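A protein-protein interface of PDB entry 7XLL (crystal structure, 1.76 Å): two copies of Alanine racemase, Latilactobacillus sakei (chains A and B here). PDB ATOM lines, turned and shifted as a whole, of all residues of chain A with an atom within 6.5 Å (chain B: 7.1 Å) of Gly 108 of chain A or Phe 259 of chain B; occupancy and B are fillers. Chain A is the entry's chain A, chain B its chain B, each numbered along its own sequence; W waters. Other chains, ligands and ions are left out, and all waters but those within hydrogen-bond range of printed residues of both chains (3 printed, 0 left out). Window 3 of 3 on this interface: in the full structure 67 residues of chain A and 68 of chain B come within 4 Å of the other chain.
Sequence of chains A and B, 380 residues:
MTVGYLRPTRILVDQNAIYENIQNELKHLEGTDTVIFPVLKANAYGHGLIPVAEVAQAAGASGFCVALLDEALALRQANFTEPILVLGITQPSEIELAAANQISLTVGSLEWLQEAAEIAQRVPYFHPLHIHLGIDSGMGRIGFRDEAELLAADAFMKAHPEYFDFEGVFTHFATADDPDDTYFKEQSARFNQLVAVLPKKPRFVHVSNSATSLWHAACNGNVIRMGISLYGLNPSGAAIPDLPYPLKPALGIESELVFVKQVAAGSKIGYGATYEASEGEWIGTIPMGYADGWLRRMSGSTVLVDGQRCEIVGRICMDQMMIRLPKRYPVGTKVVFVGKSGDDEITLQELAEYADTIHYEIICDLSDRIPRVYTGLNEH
Water W2 bridges OE1 of Gln 320 of chain B (2.6 Å) and N of Ile 89 of chain A (3.0 Å). Water W3 lies within hydrogen-bond range of OD2 of Asp 136 of chain A (2.7 Å), NZ of Lys 261 of chain B (2.8 Å) and O of Gly 143 of chain A (3.1 Å). Water W1 bridges the side-chain amide nitrogen (NE2) of Gln 320 of chain B and the guanidinium group (NH1) of Arg 141 of chain A.
Of the printed residues of chain B, Gly 108 of chain A touches Phe 259 (3.3 Å). Of the printed residues of chain B, Asp 136 of chain A touches Lys 261. Of the printed residues of chain B, Arg 145 of chain A touches Lys 261. Phe 259 of chain B touches just these residues of chain A: Gly 108, Ile 142 and Gly 143. Of the printed residues of chain A, Lys 261 of chain B touches Asp 136, Arg 141 and Arg 145. The nearest residue of chain A that does not touch Phe 259 of chain B is Arg 141 of chain A (4.1 Å).
Hydrophobic or aromatic side chains of chain B within 4 Å of the printed part of chain A: Val 258 and Phe 259. Printed residues of chain A that touch a printed residue of chain B: Ile 89, Gly 108, Asp 136, Arg 141, Ile 142, Gly 143 and Arg 145. Hydrophobic or aromatic side chains of chain A within 4 Å of the printed part of chain B: Ile 89 and Ile 142. Along chain A the printed residues that touch a printed residue of chain B span positions 89 to 145. Among the printed residues, 11 pairs touch across the chains.
NZ of Lys 261 of chain B lies within salt-bridge range of OD2 of Asp 136 of chain A, 3.995 Å away. NZ of Lys 261 of chain B is in hydrogen-bond range of O of Arg 141 of chain A (2.9 Å). O of Arg 141 of chain A is in hydrogen-bond range of OG1 of Thr 285 of chain B, at 2.6 Å. NE2 of Gln 320 of chain B lies close to NE of Arg 141 of chain A, at 3.4 Å.
N of Phe 144 of chain A is in hydrogen-bond range of O of Gly 108 of chain A. The backbone NH of Asp 136 of chain A is in hydrogen-bond range of the backbone carbonyl oxygen of Phe 144 of chain A (2.8 Å). NH1 of Arg 145 of chain A lies within salt-bridge range of OD2 of Asp 136 of chain A (3.0 Å). The backbone NH (N) of Val 258 of chain B lies within hydrogen-bond range of the backbone carbonyl oxygen (O) of Thr 285 of chain B. The backbone carbonyl oxygen (O) of Phe 259 of chain B lies within hydrogen-bond range of the backbone NH (N) of Thr 285 of chain B. The backbone carbonyl oxygen of Lys 261 of chain B is in hydrogen-bond range of the backbone NH of Ile 283 of chain B (2.7 Å).
Among the printed residues, pairs that only touch across the chains: Gly 108 of chain A with Phe 259 of chain B, Gly 143 of chain A with Phe 259 of chain B, Arg 145 of chain A with Lys 261 of chain B, Ile 89 of chain A with Val 258 of chain B, Ile 142 of chain A with Phe 259 of chain B, Ile 142 of chain A with Gln 320 of chain B and Ile 142 of chain A with Thr 285 of chain B.
No position is printed for both chains. Of the 11 pairs that touch across the chains among the printed residues, none has its exchanged pair printed and touching as well.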
ATOM      1  N   ILE A  89     -33.238  14.819   1.710  1.00  0.00           N
ATOM      2  CA  ILE A  89     -33.053  16.265   1.787  1.00  0.00           C
ATOM      3  C   ILE A  89     -34.407  16.936   1.967  1.00  0.00           C
ATOM      4  O   ILE A  89     -35.332  16.718   1.178  1.00  0.00           O
ATOM      5  CB  ILE A  89     -32.367  16.796   0.520  1.00  0.00           C
ATOM      6  CG1 ILE A  89     -30.956  16.212   0.363  1.00  0.00           C
ATOM      7  CG2 ILE A  89     -32.324  18.322   0.557  1.00  0.00           C
ATOM      8  CD1 ILE A  89     -30.035  16.503   1.540  1.00  0.00           C
ATOM      9  N   THR A 106     -31.637  15.540   7.757  1.00  0.00           N
ATOM     10  CA  THR A 106     -30.370  15.221   7.103  1.00  0.00           C
ATOM     11  C   THR A 106     -29.911  16.420   6.282  1.00  0.00           C
ATOM     12  O   THR A 106     -30.700  17.011   5.536  1.00  0.00           O
ATOM     13  CB  THR A 106     -30.524  13.986   6.198  1.00  0.00           C
ATOM     14  OG1 THR A 106     -30.651  12.805   6.999  1.00  0.00           O
ATOM     15  CG2 THR A 106     -29.313  13.819   5.280  1.00  0.00           C
ATOM     16  N   VAL A 107     -28.636  16.790   6.431  1.00  0.00           N
ATOM     17  CA  VAL A 107     -28.064  17.940   5.746  1.00  0.00           C
ATOM     18  C   VAL A 107     -26.777  17.484   5.090  1.00  0.00           C
ATOM     19  O   VAL A 107     -25.937  16.858   5.746  1.00  0.00           O
ATOM     20  CB  VAL A 107     -27.784  19.107   6.714  1.00  0.00           C
ATOM     21  CG1 VAL A 107     -27.023  20.210   6.001  1.00  0.00           C
ATOM     22  CG2 VAL A 107     -29.073  19.622   7.293  1.00  0.00           C
ATOM     23  N   GLY A 108     -26.627  17.780   3.801  1.00  0.00           N
ATOM     24  CA  GLY A 108     -25.467  17.269   3.087  1.00  0.00           C
ATOM     25  C   GLY A 108     -24.550  18.331   2.516  1.00  0.00           C
ATOM     26  O   GLY A 108     -23.628  18.009   1.752  1.00  0.00           O
ATOM     27  N   SER A 109     -24.786  19.597   2.871  1.00  0.00           N
ATOM     28  CA  SER A 109     -24.010  20.685   2.286  1.00  0.00           C
ATOM     29  C   SER A 109     -23.994  21.893   3.214  1.00  0.00           C
ATOM     30  O   SER A 109     -24.946  22.139   3.965  1.00  0.00           O
ATOM     31  CB  SER A 109     -24.558  21.084   0.916  1.00  0.00           C
ATOM     32  OG  SER A 109     -25.843  21.666   1.058  1.00  0.00           O
ATOM     33  N   LEU A 110     -22.895  22.657   3.144  1.00  0.00           N
ATOM     34  CA  LEU A 110     -22.842  23.926   3.859  1.00  0.00           C
ATOM     35  C   LEU A 110     -23.876  24.907   3.315  1.00  0.00           C
ATOM     36  O   LEU A 110     -24.448  25.697   4.073  1.00  0.00           O
ATOM     37  CB  LEU A 110     -21.435  24.519   3.767  1.00  0.00           C
ATOM     38  CG  LEU A 110     -21.258  25.960   4.261  1.00  0.00           C
ATOM     39  CD1 LEU A 110     -21.571  26.100   5.746  1.00  0.00           C
ATOM     40  CD2 LEU A 110     -19.842  26.438   3.970  1.00  0.00           C
ATOM     41  N   TRP A 112     -26.900  24.380   2.319  1.00  0.00           N
ATOM     42  CA  TRP A 112     -28.181  24.170   2.985  1.00  0.00           C
ATOM     43  C   TRP A 112     -28.220  24.925   4.308  1.00  0.00           C
ATOM     44  O   TRP A 112     -29.172  25.655   4.594  1.00  0.00           O
ATOM     45  CB  TRP A 112     -28.423  22.670   3.197  1.00  0.00           C
ATOM     46  CG  TRP A 112     -29.815  22.357   3.706  1.00  0.00           C
ATOM     47  CD1 TRP A 112     -30.881  21.928   2.962  1.00  0.00           C
ATOM     48  CD2 TRP A 112     -30.286  22.458   5.056  1.00  0.00           C
ATOM     49  NE1 TRP A 112     -31.980  21.750   3.771  1.00  0.00           N
ATOM     50  CE2 TRP A 112     -31.645  22.077   5.056  1.00  0.00           C
ATOM     51  CE3 TRP A 112     -29.693  22.835   6.265  1.00  0.00           C
ATOM     52  CZ2 TRP A 112     -32.421  22.062   6.229  1.00  0.00           C
ATOM     53  CZ3 TRP A 112     -30.453  22.820   7.415  1.00  0.00           C
ATOM     54  CH2 TRP A 112     -31.805  22.438   7.391  1.00  0.00           C
ATOM     55  N   HIS A 132     -28.582  16.096  11.399  1.00  0.00           N
ATOM     56  CA  HIS A 132     -27.630  15.025  11.101  1.00  0.00           C
ATOM     57  C   HIS A 132     -26.890  15.389   9.818  1.00  0.00           C
ATOM     58  O   HIS A 132     -27.520  15.615   8.780  1.00  0.00           O
ATOM     59  CB  HIS A 132     -28.339  13.668  10.958  1.00  0.00           C
ATOM     60  CG  HIS A 132     -28.909  13.139  12.245  1.00  0.00           C
ATOM     61  ND1 HIS A 132     -28.723  11.836  12.666  1.00  0.00           N
ATOM     62  CD2 HIS A 132     -29.648  13.741  13.208  1.00  0.00           C
ATOM     63  CE1 HIS A 132     -29.320  11.663  13.834  1.00  0.00           C
ATOM     64  NE2 HIS A 132     -29.891  12.804  14.184  1.00  0.00           N
ATOM     65  N   LEU A 133     -25.557  15.451   9.883  1.00  0.00           N
ATOM     66  CA  LEU A 133     -24.752  15.663   8.684  1.00  0.00           C
ATOM     67  C   LEU A 133     -24.606  14.335   7.956  1.00  0.00           C
ATOM     68  O   LEU A 133     -24.119  13.358   8.535  1.00  0.00           O
ATOM     69  CB  LEU A 133     -23.374  16.228   9.042  1.00  0.00           C
ATOM     70  CG  LEU A 133     -23.350  17.590   9.740  1.00  0.00           C
ATOM     71  CD1 LEU A 133     -21.900  18.045   9.919  1.00  0.00           C
ATOM     72  CD2 LEU A 133     -24.141  18.645   8.986  1.00  0.00           C
ATOM     73  N   GLY A 134     -25.081  14.283   6.709  1.00  0.00           N
ATOM     74  CA  GLY A 134     -24.913  13.106   5.876  1.00  0.00           C
ATOM     75  C   GLY A 134     -23.584  13.174   5.152  1.00  0.00           C
ATOM     76  O   GLY A 134     -23.276  14.167   4.487  1.00  0.00           O
ATOM     77  N   ILE A 135     -22.787  12.126   5.311  1.00  0.00           N
ATOM     78  CA  ILE A 135     -21.494  12.013   4.649  1.00  0.00           C
ATOM     79  C   ILE A 135     -21.647  11.012   3.519  1.00  0.00           C
ATOM     80  O   ILE A 135     -22.163   9.905   3.728  1.00  0.00           O
ATOM     81  CB  ILE A 135     -20.396  11.585   5.636  1.00  0.00           C
ATOM     82  CG1 ILE A 135     -20.146  12.709   6.648  1.00  0.00           C
ATOM     83  CG2 ILE A 135     -19.102  11.176   4.893  1.00  0.00           C
ATOM     84  CD1 ILE A 135     -19.052  12.387   7.623  1.00  0.00           C
ATOM     85  N   ASP A 136     -21.220  11.409   2.321  1.00  0.00           N
ATOM     86  CA  ASP A 136     -21.190  10.540   1.147  1.00  0.00           C
ATOM     87  C   ASP A 136     -19.822   9.874   1.135  1.00  0.00           C
ATOM     88  O   ASP A 136     -18.814  10.498   0.784  1.00  0.00           O
ATOM     89  CB  ASP A 136     -21.447  11.358  -0.115  1.00  0.00           C
ATOM     90  CG  ASP A 136     -21.434  10.528  -1.395  1.00  0.00           C
ATOM     91  OD1 ASP A 136     -21.137   9.309  -1.374  1.00  0.00           O
ATOM     92  OD2 ASP A 136     -21.737  11.128  -2.445  1.00  0.00           O
ATOM     93  N   ARG A 141     -25.019   9.533  -3.461  1.00  0.00           N
ATOM     94  CA  ARG A 141     -26.413   9.964  -3.444  1.00  0.00           C
ATOM     95  C   ARG A 141     -26.524  11.398  -2.942  1.00  0.00           C
ATOM     96  O   ARG A 141     -26.666  12.336  -3.736  1.00  0.00           O
ATOM     97  CB  ARG A 141     -27.227   9.008  -2.576  1.00  0.00           C
ATOM     98  CG  ARG A 141     -28.725   9.283  -2.530  1.00  0.00           C
ATOM     99  CD  ARG A 141     -29.485   8.006  -2.150  1.00  0.00           C
ATOM    100  NE  ARG A 141     -29.262   7.621  -0.753  1.00  0.00           N
ATOM    101  CZ  ARG A 141     -29.873   6.604  -0.146  1.00  0.00           C
ATOM    102  NH1 ARG A 141     -29.628   6.347   1.136  1.00  0.00           N
ATOM    103  NH2 ARG A 141     -30.729   5.840  -0.814  1.00  0.00           N
ATOM    104  N   ILE A 142     -26.428  11.581  -1.624  1.00  0.00           N
ATOM    105  CA  ILE A 142     -26.313  12.900  -1.015  1.00  0.00           C
ATOM    106  C   ILE A 142     -25.202  12.873   0.028  1.00  0.00           C
ATOM    107  O   ILE A 142     -24.771  11.811   0.491  1.00  0.00           O
ATOM    108  CB  ILE A 142     -27.645  13.364  -0.376  1.00  0.00           C
ATOM    109  CG1 ILE A 142     -28.070  12.399   0.726  1.00  0.00           C
ATOM    110  CG2 ILE A 142     -28.722  13.464  -1.454  1.00  0.00           C
ATOM    111  CD1 ILE A 142     -29.395  12.779   1.395  1.00  0.00           C
ATOM    112  N   GLY A 143     -24.721  14.058   0.379  1.00  0.00           N
ATOM    113  CA  GLY A 143     -23.831  14.209   1.513  1.00  0.00           C
ATOM    114  C   GLY A 143     -22.484  14.814   1.144  1.00  0.00           C
ATOM    115  O   GLY A 143     -22.095  14.908  -0.020  1.00  0.00           O
ATOM    116  N   PHE A 144     -21.771  15.212   2.197  1.00  0.00           N
ATOM    117  CA  PHE A 144     -20.444  15.797   2.057  1.00  0.00           C
ATOM    118  C   PHE A 144     -19.476  14.771   1.503  1.00  0.00           C
ATOM    119  O   PHE A 144     -19.539  13.586   1.850  1.00  0.00           O
ATOM    120  CB  PHE A 144     -19.924  16.298   3.407  1.00  0.00           C
ATOM    121  CG  PHE A 144     -20.778  17.363   4.031  1.00  0.00           C
ATOM    122  CD1 PHE A 144     -20.527  18.705   3.788  1.00  0.00           C
ATOM    123  CD2 PHE A 144     -21.844  17.024   4.845  1.00  0.00           C
ATOM    124  CE1 PHE A 144     -21.323  19.693   4.369  1.00  0.00           C
ATOM    125  CE2 PHE A 144     -22.646  18.006   5.413  1.00  0.00           C
ATOM    126  CZ  PHE A 144     -22.389  19.333   5.171  1.00  0.00           C
ATOM    127  N   ARG A 145     -18.541  15.248   0.672  1.00  0.00           N
ATOM    128  CA  ARG A 145     -17.577  14.379   0.016  1.00  0.00           C
ATOM    129  C   ARG A 145     -16.135  14.807   0.282  1.00  0.00           C
ATOM    130  O   ARG A 145     -15.214  14.244  -0.320  1.00  0.00           O
ATOM    131  CB  ARG A 145     -17.859  14.317  -1.498  1.00  0.00           C
ATOM    132  CG  ARG A 145     -19.038  13.389  -1.857  1.00  0.00           C
ATOM    133  CD  ARG A 145     -19.434  13.423  -3.342  1.00  0.00           C
ATOM    134  NE  ARG A 145     -18.441  12.831  -4.248  1.00  0.00           N
ATOM    135  CZ  ARG A 145     -18.400  11.551  -4.612  1.00  0.00           C
ATOM    136  NH1 ARG A 145     -19.283  10.686  -4.131  1.00  0.00           N
ATOM    137  NH2 ARG A 145     -17.463  11.127  -5.459  1.00  0.00           N
ATOM    138  N   GLU A 149     -15.406  20.848   3.503  1.00  0.00           N
ATOM    139  CA  GLU A 149     -16.779  21.327   3.627  1.00  0.00           C
ATOM    140  C   GLU A 149     -17.448  20.750   4.868  1.00  0.00           C
ATOM    141  O   GLU A 149     -18.260  21.427   5.511  1.00  0.00           O
ATOM    142  CB  GLU A 149     -17.586  20.994   2.377  1.00  0.00           C
ATOM    143  CG  GLU A 149     -18.907  21.777   2.314  1.00  0.00           C
ATOM    144  CD  GLU A 149     -19.889  21.212   1.313  1.00  0.00           C
ATOM    145  OE1 GLU A 149     -19.521  20.271   0.579  1.00  0.00           O
ATOM    146  OE2 GLU A 149     -21.035  21.703   1.272  1.00  0.00           O
ATOM    147  N   GLU B 256     -37.839  18.197  -8.477  1.00  0.00           N
ATOM    148  CA  GLU B 256     -36.762  19.183  -8.402  1.00  0.00           C
ATOM    149  C   GLU B 256     -35.475  18.481  -8.020  1.00  0.00           C
ATOM    150  O   GLU B 256     -35.494  17.428  -7.383  1.00  0.00           O
ATOM    151  CB  GLU B 256     -37.025  20.274  -7.357  1.00  0.00           C
ATOM    152  CG  GLU B 256     -38.100  21.255  -7.686  1.00  0.00           C
ATOM    153  CD  GLU B 256     -38.345  22.202  -6.527  1.00  0.00           C
ATOM    154  OE1 GLU B 256     -37.613  22.096  -5.511  1.00  0.00           O
ATOM    155  OE2 GLU B 256     -39.267  23.038  -6.627  1.00  0.00           O
ATOM    156  N   LEU B 257     -34.341  19.086  -8.387  1.00  0.00           N
ATOM    157  CA  LEU B 257     -33.071  18.634  -7.840  1.00  0.00           C
ATOM    158  C   LEU B 257     -32.991  18.993  -6.361  1.00  0.00           C
ATOM    159  O   LEU B 257     -33.283  20.128  -5.977  1.00  0.00           O
ATOM    160  CB  LEU B 257     -31.905  19.273  -8.594  1.00  0.00           C
ATOM    161  CG  LEU B 257     -31.910  19.108 -10.107  1.00  0.00           C
ATOM    162  CD1 LEU B 257     -30.768  19.890 -10.741  1.00  0.00           C
ATOM    163  CD2 LEU B 257     -31.792  17.628 -10.443  1.00  0.00           C
ATOM    164  N   VAL B 258     -32.576  18.036  -5.534  1.00  0.00           N
ATOM    165  CA  VAL B 258     -32.331  18.298  -4.119  1.00  0.00           C
ATOM    166  C   VAL B 258     -30.854  18.240  -3.759  1.00  0.00           C
ATOM    167  O   VAL B 258     -30.492  18.593  -2.623  1.00  0.00           O
ATOM    168  CB  VAL B 258     -33.135  17.341  -3.210  1.00  0.00           C
ATOM    169  CG1 VAL B 258     -34.635  17.583  -3.383  1.00  0.00           C
ATOM    170  CG2 VAL B 258     -32.778  15.884  -3.499  1.00  0.00           C
ATOM    171  N   PHE B 259     -29.989  17.825  -4.680  1.00  0.00           N
ATOM    172  CA  PHE B 259     -28.559  17.749  -4.425  1.00  0.00           C
ATOM    173  C   PHE B 259     -27.848  17.766  -5.765  1.00  0.00           C
ATOM    174  O   PHE B 259     -28.302  17.127  -6.715  1.00  0.00           O
ATOM    175  CB  PHE B 259     -28.175  16.490  -3.636  1.00  0.00           C
ATOM    176  CG  PHE B 259     -26.945  16.661  -2.801  1.00  0.00           C
ATOM    177  CD1 PHE B 259     -27.028  17.203  -1.519  1.00  0.00           C
ATOM    178  CD2 PHE B 259     -25.699  16.318  -3.300  1.00  0.00           C
ATOM    179  CE1 PHE B 259     -25.889  17.380  -0.750  1.00  0.00           C
ATOM    180  CE2 PHE B 259     -24.545  16.491  -2.539  1.00  0.00           C
ATOM    181  CZ  PHE B 259     -24.637  17.020  -1.260  1.00  0.00           C
ATOM    182  N   VAL B 260     -26.744  18.507  -5.838  1.00  0.00           N
ATOM    183  CA  VAL B 260     -25.968  18.632  -7.067  1.00  0.00           C
ATOM    184  C   VAL B 260     -24.492  18.617  -6.704  1.00  0.00           C
ATOM    185  O   VAL B 260     -24.064  19.337  -5.794  1.00  0.00           O
ATOM    186  CB  VAL B 260     -26.305  19.914  -7.855  1.00  0.00           C
ATOM    187  CG1 VAL B 260     -25.385  20.031  -9.065  1.00  0.00           C
ATOM    188  CG2 VAL B 260     -27.775  19.933  -8.287  1.00  0.00           C
ATOM    189  N   LYS B 261     -23.718  17.791  -7.404  1.00  0.00           N
ATOM    190  CA  LYS B 261     -22.289  17.682  -7.145  1.00  0.00           C
ATOM    191  C   LYS B 261     -21.558  17.337  -8.433  1.00  0.00           C
ATOM    192  O   LYS B 261     -22.129  16.765  -9.365  1.00  0.00           O
ATOM    193  CB  LYS B 261     -21.986  16.610  -6.097  1.00  0.00           C
ATOM    194  CG  LYS B 261     -22.634  15.269  -6.410  1.00  0.00           C
ATOM    195  CD  LYS B 261     -22.036  14.169  -5.557  1.00  0.00           C
ATOM    196  CE  LYS B 261     -22.809  12.853  -5.683  1.00  0.00           C
ATOM    197  NZ  LYS B 261     -24.179  12.907  -5.059  1.00  0.00           N
ATOM    198  N   ILE B 283     -23.690  15.360 -11.134  1.00  0.00           N
ATOM    199  CA  ILE B 283     -24.689  14.389 -10.699  1.00  0.00           C
ATOM    200  C   ILE B 283     -25.763  15.123  -9.915  1.00  0.00           C
ATOM    201  O   ILE B 283     -25.458  15.835  -8.952  1.00  0.00           O
ATOM    202  CB  ILE B 283     -24.058  13.268  -9.853  1.00  0.00           C
ATOM    203  CG1 ILE B 283     -22.912  12.585 -10.622  1.00  0.00           C
ATOM    204  CG2 ILE B 283     -25.116  12.251  -9.439  1.00  0.00           C
ATOM    205  CD1 ILE B 283     -23.375  11.692 -11.761  1.00  0.00           C
ATOM    206  N   GLY B 284     -27.015  14.954 -10.322  1.00  0.00           N
ATOM    207  CA  GLY B 284     -28.152  15.524  -9.610  1.00  0.00           C
ATOM    208  C   GLY B 284     -28.926  14.423  -8.909  1.00  0.00           C
ATOM    209  O   GLY B 284     -29.087  13.328  -9.452  1.00  0.00           O
ATOM    210  N   THR B 285     -29.415  14.720  -7.708  1.00  0.00           N
ATOM    211  CA  THR B 285     -30.239  13.780  -6.961  1.00  0.00           C
ATOM    212  C   THR B 285     -31.676  14.291  -6.932  1.00  0.00           C
ATOM    213  O   THR B 285     -31.913  15.489  -6.759  1.00  0.00           O
ATOM    214  CB  THR B 285     -29.682  13.579  -5.542  1.00  0.00           C
ATOM    215  OG1 THR B 285     -28.290  13.211  -5.630  1.00  0.00           O
ATOM    216  CG2 THR B 285     -30.446  12.481  -4.797  1.00  0.00           C
ATOM    217  N   ILE B 286     -32.626  13.387  -7.148  1.00  0.00           N
ATOM    218  CA  ILE B 286     -34.038  13.721  -7.306  1.00  0.00           C
ATOM    219  C   ILE B 286     -34.817  12.948  -6.256  1.00  0.00           C
ATOM    220  O   ILE B 286     -34.603  11.744  -6.110  1.00  0.00           O
ATOM    221  CB  ILE B 286     -34.562  13.373  -8.714  1.00  0.00           C
ATOM    222  CG1 ILE B 286     -33.846  14.193  -9.778  1.00  0.00           C
ATOM    223  CG2 ILE B 286     -36.064  13.589  -8.806  1.00  0.00           C
ATOM    224  CD1 ILE B 286     -33.857  13.519 -11.126  1.00  0.00           C
ATOM    225  N   PRO B 287     -35.741  13.586  -5.516  1.00  0.00           N
ATOM    226  CA  PRO B 287     -36.549  12.894  -4.484  1.00  0.00           C
ATOM    227  C   PRO B 287     -37.737  12.155  -5.094  1.00  0.00           C
ATOM    228  O   PRO B 287     -38.910  12.501  -4.918  1.00  0.00           O
ATOM    229  CB  PRO B 287     -36.976  14.051  -3.577  1.00  0.00           C
ATOM    230  CG  PRO B 287     -37.158  15.177  -4.508  1.00  0.00           C
ATOM    231  CD  PRO B 287     -36.029  15.032  -5.541  1.00  0.00           C
ATOM    232  N   GLN B 320     -35.156   7.920  -3.896  1.00  0.00           N
ATOM    233  CA  GLN B 320     -34.273   8.863  -4.558  1.00  0.00           C
ATOM    234  C   GLN B 320     -33.663   8.208  -5.787  1.00  0.00           C
ATOM    235  O   GLN B 320     -33.564   6.987  -5.875  1.00  0.00           O
ATOM    236  CB  GLN B 320     -33.145   9.336  -3.628  1.00  0.00           C
ATOM    237  CG  GLN B 320     -33.641   9.958  -2.330  1.00  0.00           C
ATOM    238  CD  GLN B 320     -32.526  10.180  -1.341  1.00  0.00           C
ATOM    239  OE1 GLN B 320     -31.874  11.222  -1.359  1.00  0.00           O
ATOM    240  NE2 GLN B 320     -32.305   9.208  -0.462  1.00  0.00           N
ATOM    241  N   LEU B 325     -26.237  15.343 -15.126  1.00  0.00           N
ATOM    242  CA  LEU B 325     -26.475  16.717 -15.541  1.00  0.00           C
ATOM    243  C   LEU B 325     -25.425  17.138 -16.569  1.00  0.00           C
ATOM    244  O   LEU B 325     -24.265  16.731 -16.468  1.00  0.00           O
ATOM    245  CB  LEU B 325     -26.417  17.659 -14.341  1.00  0.00           C
ATOM    246  CG  LEU B 325     -27.528  17.496 -13.301  1.00  0.00           C
ATOM    247  CD1 LEU B 325     -27.242  18.318 -12.072  1.00  0.00           C
ATOM    248  CD2 LEU B 325     -28.860  17.916 -13.898  1.00  0.00           C
ATOM    249  N   ARG B 328     -23.481  22.276 -14.124  1.00  0.00           N
ATOM    250  CA  ARG B 328     -24.013  22.585 -12.806  1.00  0.00           C
ATOM    251  C   ARG B 328     -25.358  23.287 -12.932  1.00  0.00           C
ATOM    252  O   ARG B 328     -25.526  24.196 -13.754  1.00  0.00           O
ATOM    253  CB  ARG B 328     -23.032  23.458 -12.021  1.00  0.00           C
ATOM    254  CG  ARG B 328     -23.648  24.160 -10.815  1.00  0.00           C
ATOM    255  CD  ARG B 328     -22.647  24.325  -9.667  1.00  0.00           C
ATOM    256  NE  ARG B 328     -23.064  23.559  -8.494  1.00  0.00           N
ATOM    257  CZ  ARG B 328     -22.264  23.226  -7.486  1.00  0.00           C
ATOM    258  NH1 ARG B 328     -20.991  23.595  -7.494  1.00  0.00           N
ATOM    259  NH2 ARG B 328     -22.740  22.519  -6.468  1.00  0.00           N
ATOM    260  N   TYR B 329     -26.322  22.847 -12.128  1.00  0.00           N
ATOM    261  CA  TYR B 329     -27.606  23.501 -11.975  1.00  0.00           C
ATOM    262  C   TYR B 329     -27.848  23.756 -10.498  1.00  0.00           C
ATOM    263  O   TYR B 329     -27.348  23.012  -9.646  1.00  0.00           O
ATOM    264  CB  TYR B 329     -28.755  22.652 -12.546  1.00  0.00           C
ATOM    265  CG  TYR B 329     -28.878  22.770 -14.047  1.00  0.00           C
ATOM    266  CD1 TYR B 329     -28.181  21.912 -14.891  1.00  0.00           C
ATOM    267  CD2 TYR B 329     -29.695  23.738 -14.619  1.00  0.00           C
ATOM    268  CE1 TYR B 329     -28.288  22.021 -16.268  1.00  0.00           C
ATOM    269  CE2 TYR B 329     -29.808  23.856 -15.992  1.00  0.00           C
ATOM    270  CZ  TYR B 329     -29.104  22.997 -16.811  1.00  0.00           C
ATOM    271  OH  TYR B 329     -29.224  23.120 -18.178  1.00  0.00           O
ATOM    272  N   PRO B 330     -28.593  24.802 -10.165  1.00  0.00           N
ATOM    273  CA  PRO B 330     -28.922  25.049  -8.758  1.00  0.00           C
ATOM    274  C   PRO B 330     -29.853  23.981  -8.213  1.00  0.00           C
ATOM    275  O   PRO B 330     -30.712  23.452  -8.921  1.00  0.00           O
ATOM    276  CB  PRO B 330     -29.629  26.409  -8.786  1.00  0.00           C
ATOM    277  CG  PRO B 330     -29.383  26.969 -10.142  1.00  0.00           C
ATOM    278  CD  PRO B 330     -29.160  25.828 -11.054  1.00  0.00           C
ATOM    279  N   VAL B 331     -29.683  23.684  -6.924  1.00  0.00           N
ATOM    280  CA  VAL B 331     -30.695  22.915  -6.215  1.00  0.00           C
ATOM    281  C   VAL B 331     -32.026  23.653  -6.301  1.00  0.00           C
ATOM    282  O   VAL B 331     -32.081  24.888  -6.232  1.00  0.00           O
ATOM    283  CB  VAL B 331     -30.250  22.666  -4.763  1.00  0.00           C
ATOM    284  CG1 VAL B 331     -31.403  22.193  -3.909  1.00  0.00           C
ATOM    285  CG2 VAL B 331     -29.134  21.634  -4.745  1.00  0.00           C
ATOM    286  N   GLY B 332     -33.105  22.896  -6.506  1.00  0.00           N
ATOM    287  CA  GLY B 332     -34.409  23.459  -6.770  1.00  0.00           C
ATOM    288  C   GLY B 332     -34.774  23.542  -8.240  1.00  0.00           C
ATOM    289  O   GLY B 332     -35.921  23.876  -8.557  1.00  0.00           O
HETATM  290  O   HOH W   1     -32.515   7.548   2.279  1.00  0.00           O
HETATM  291  O   HOH W   2     -33.387  13.343  -0.949  1.00  0.00           O
HETATM  292  O   HOH W   3     -23.258  13.308  -2.434  1.00  0.00           O
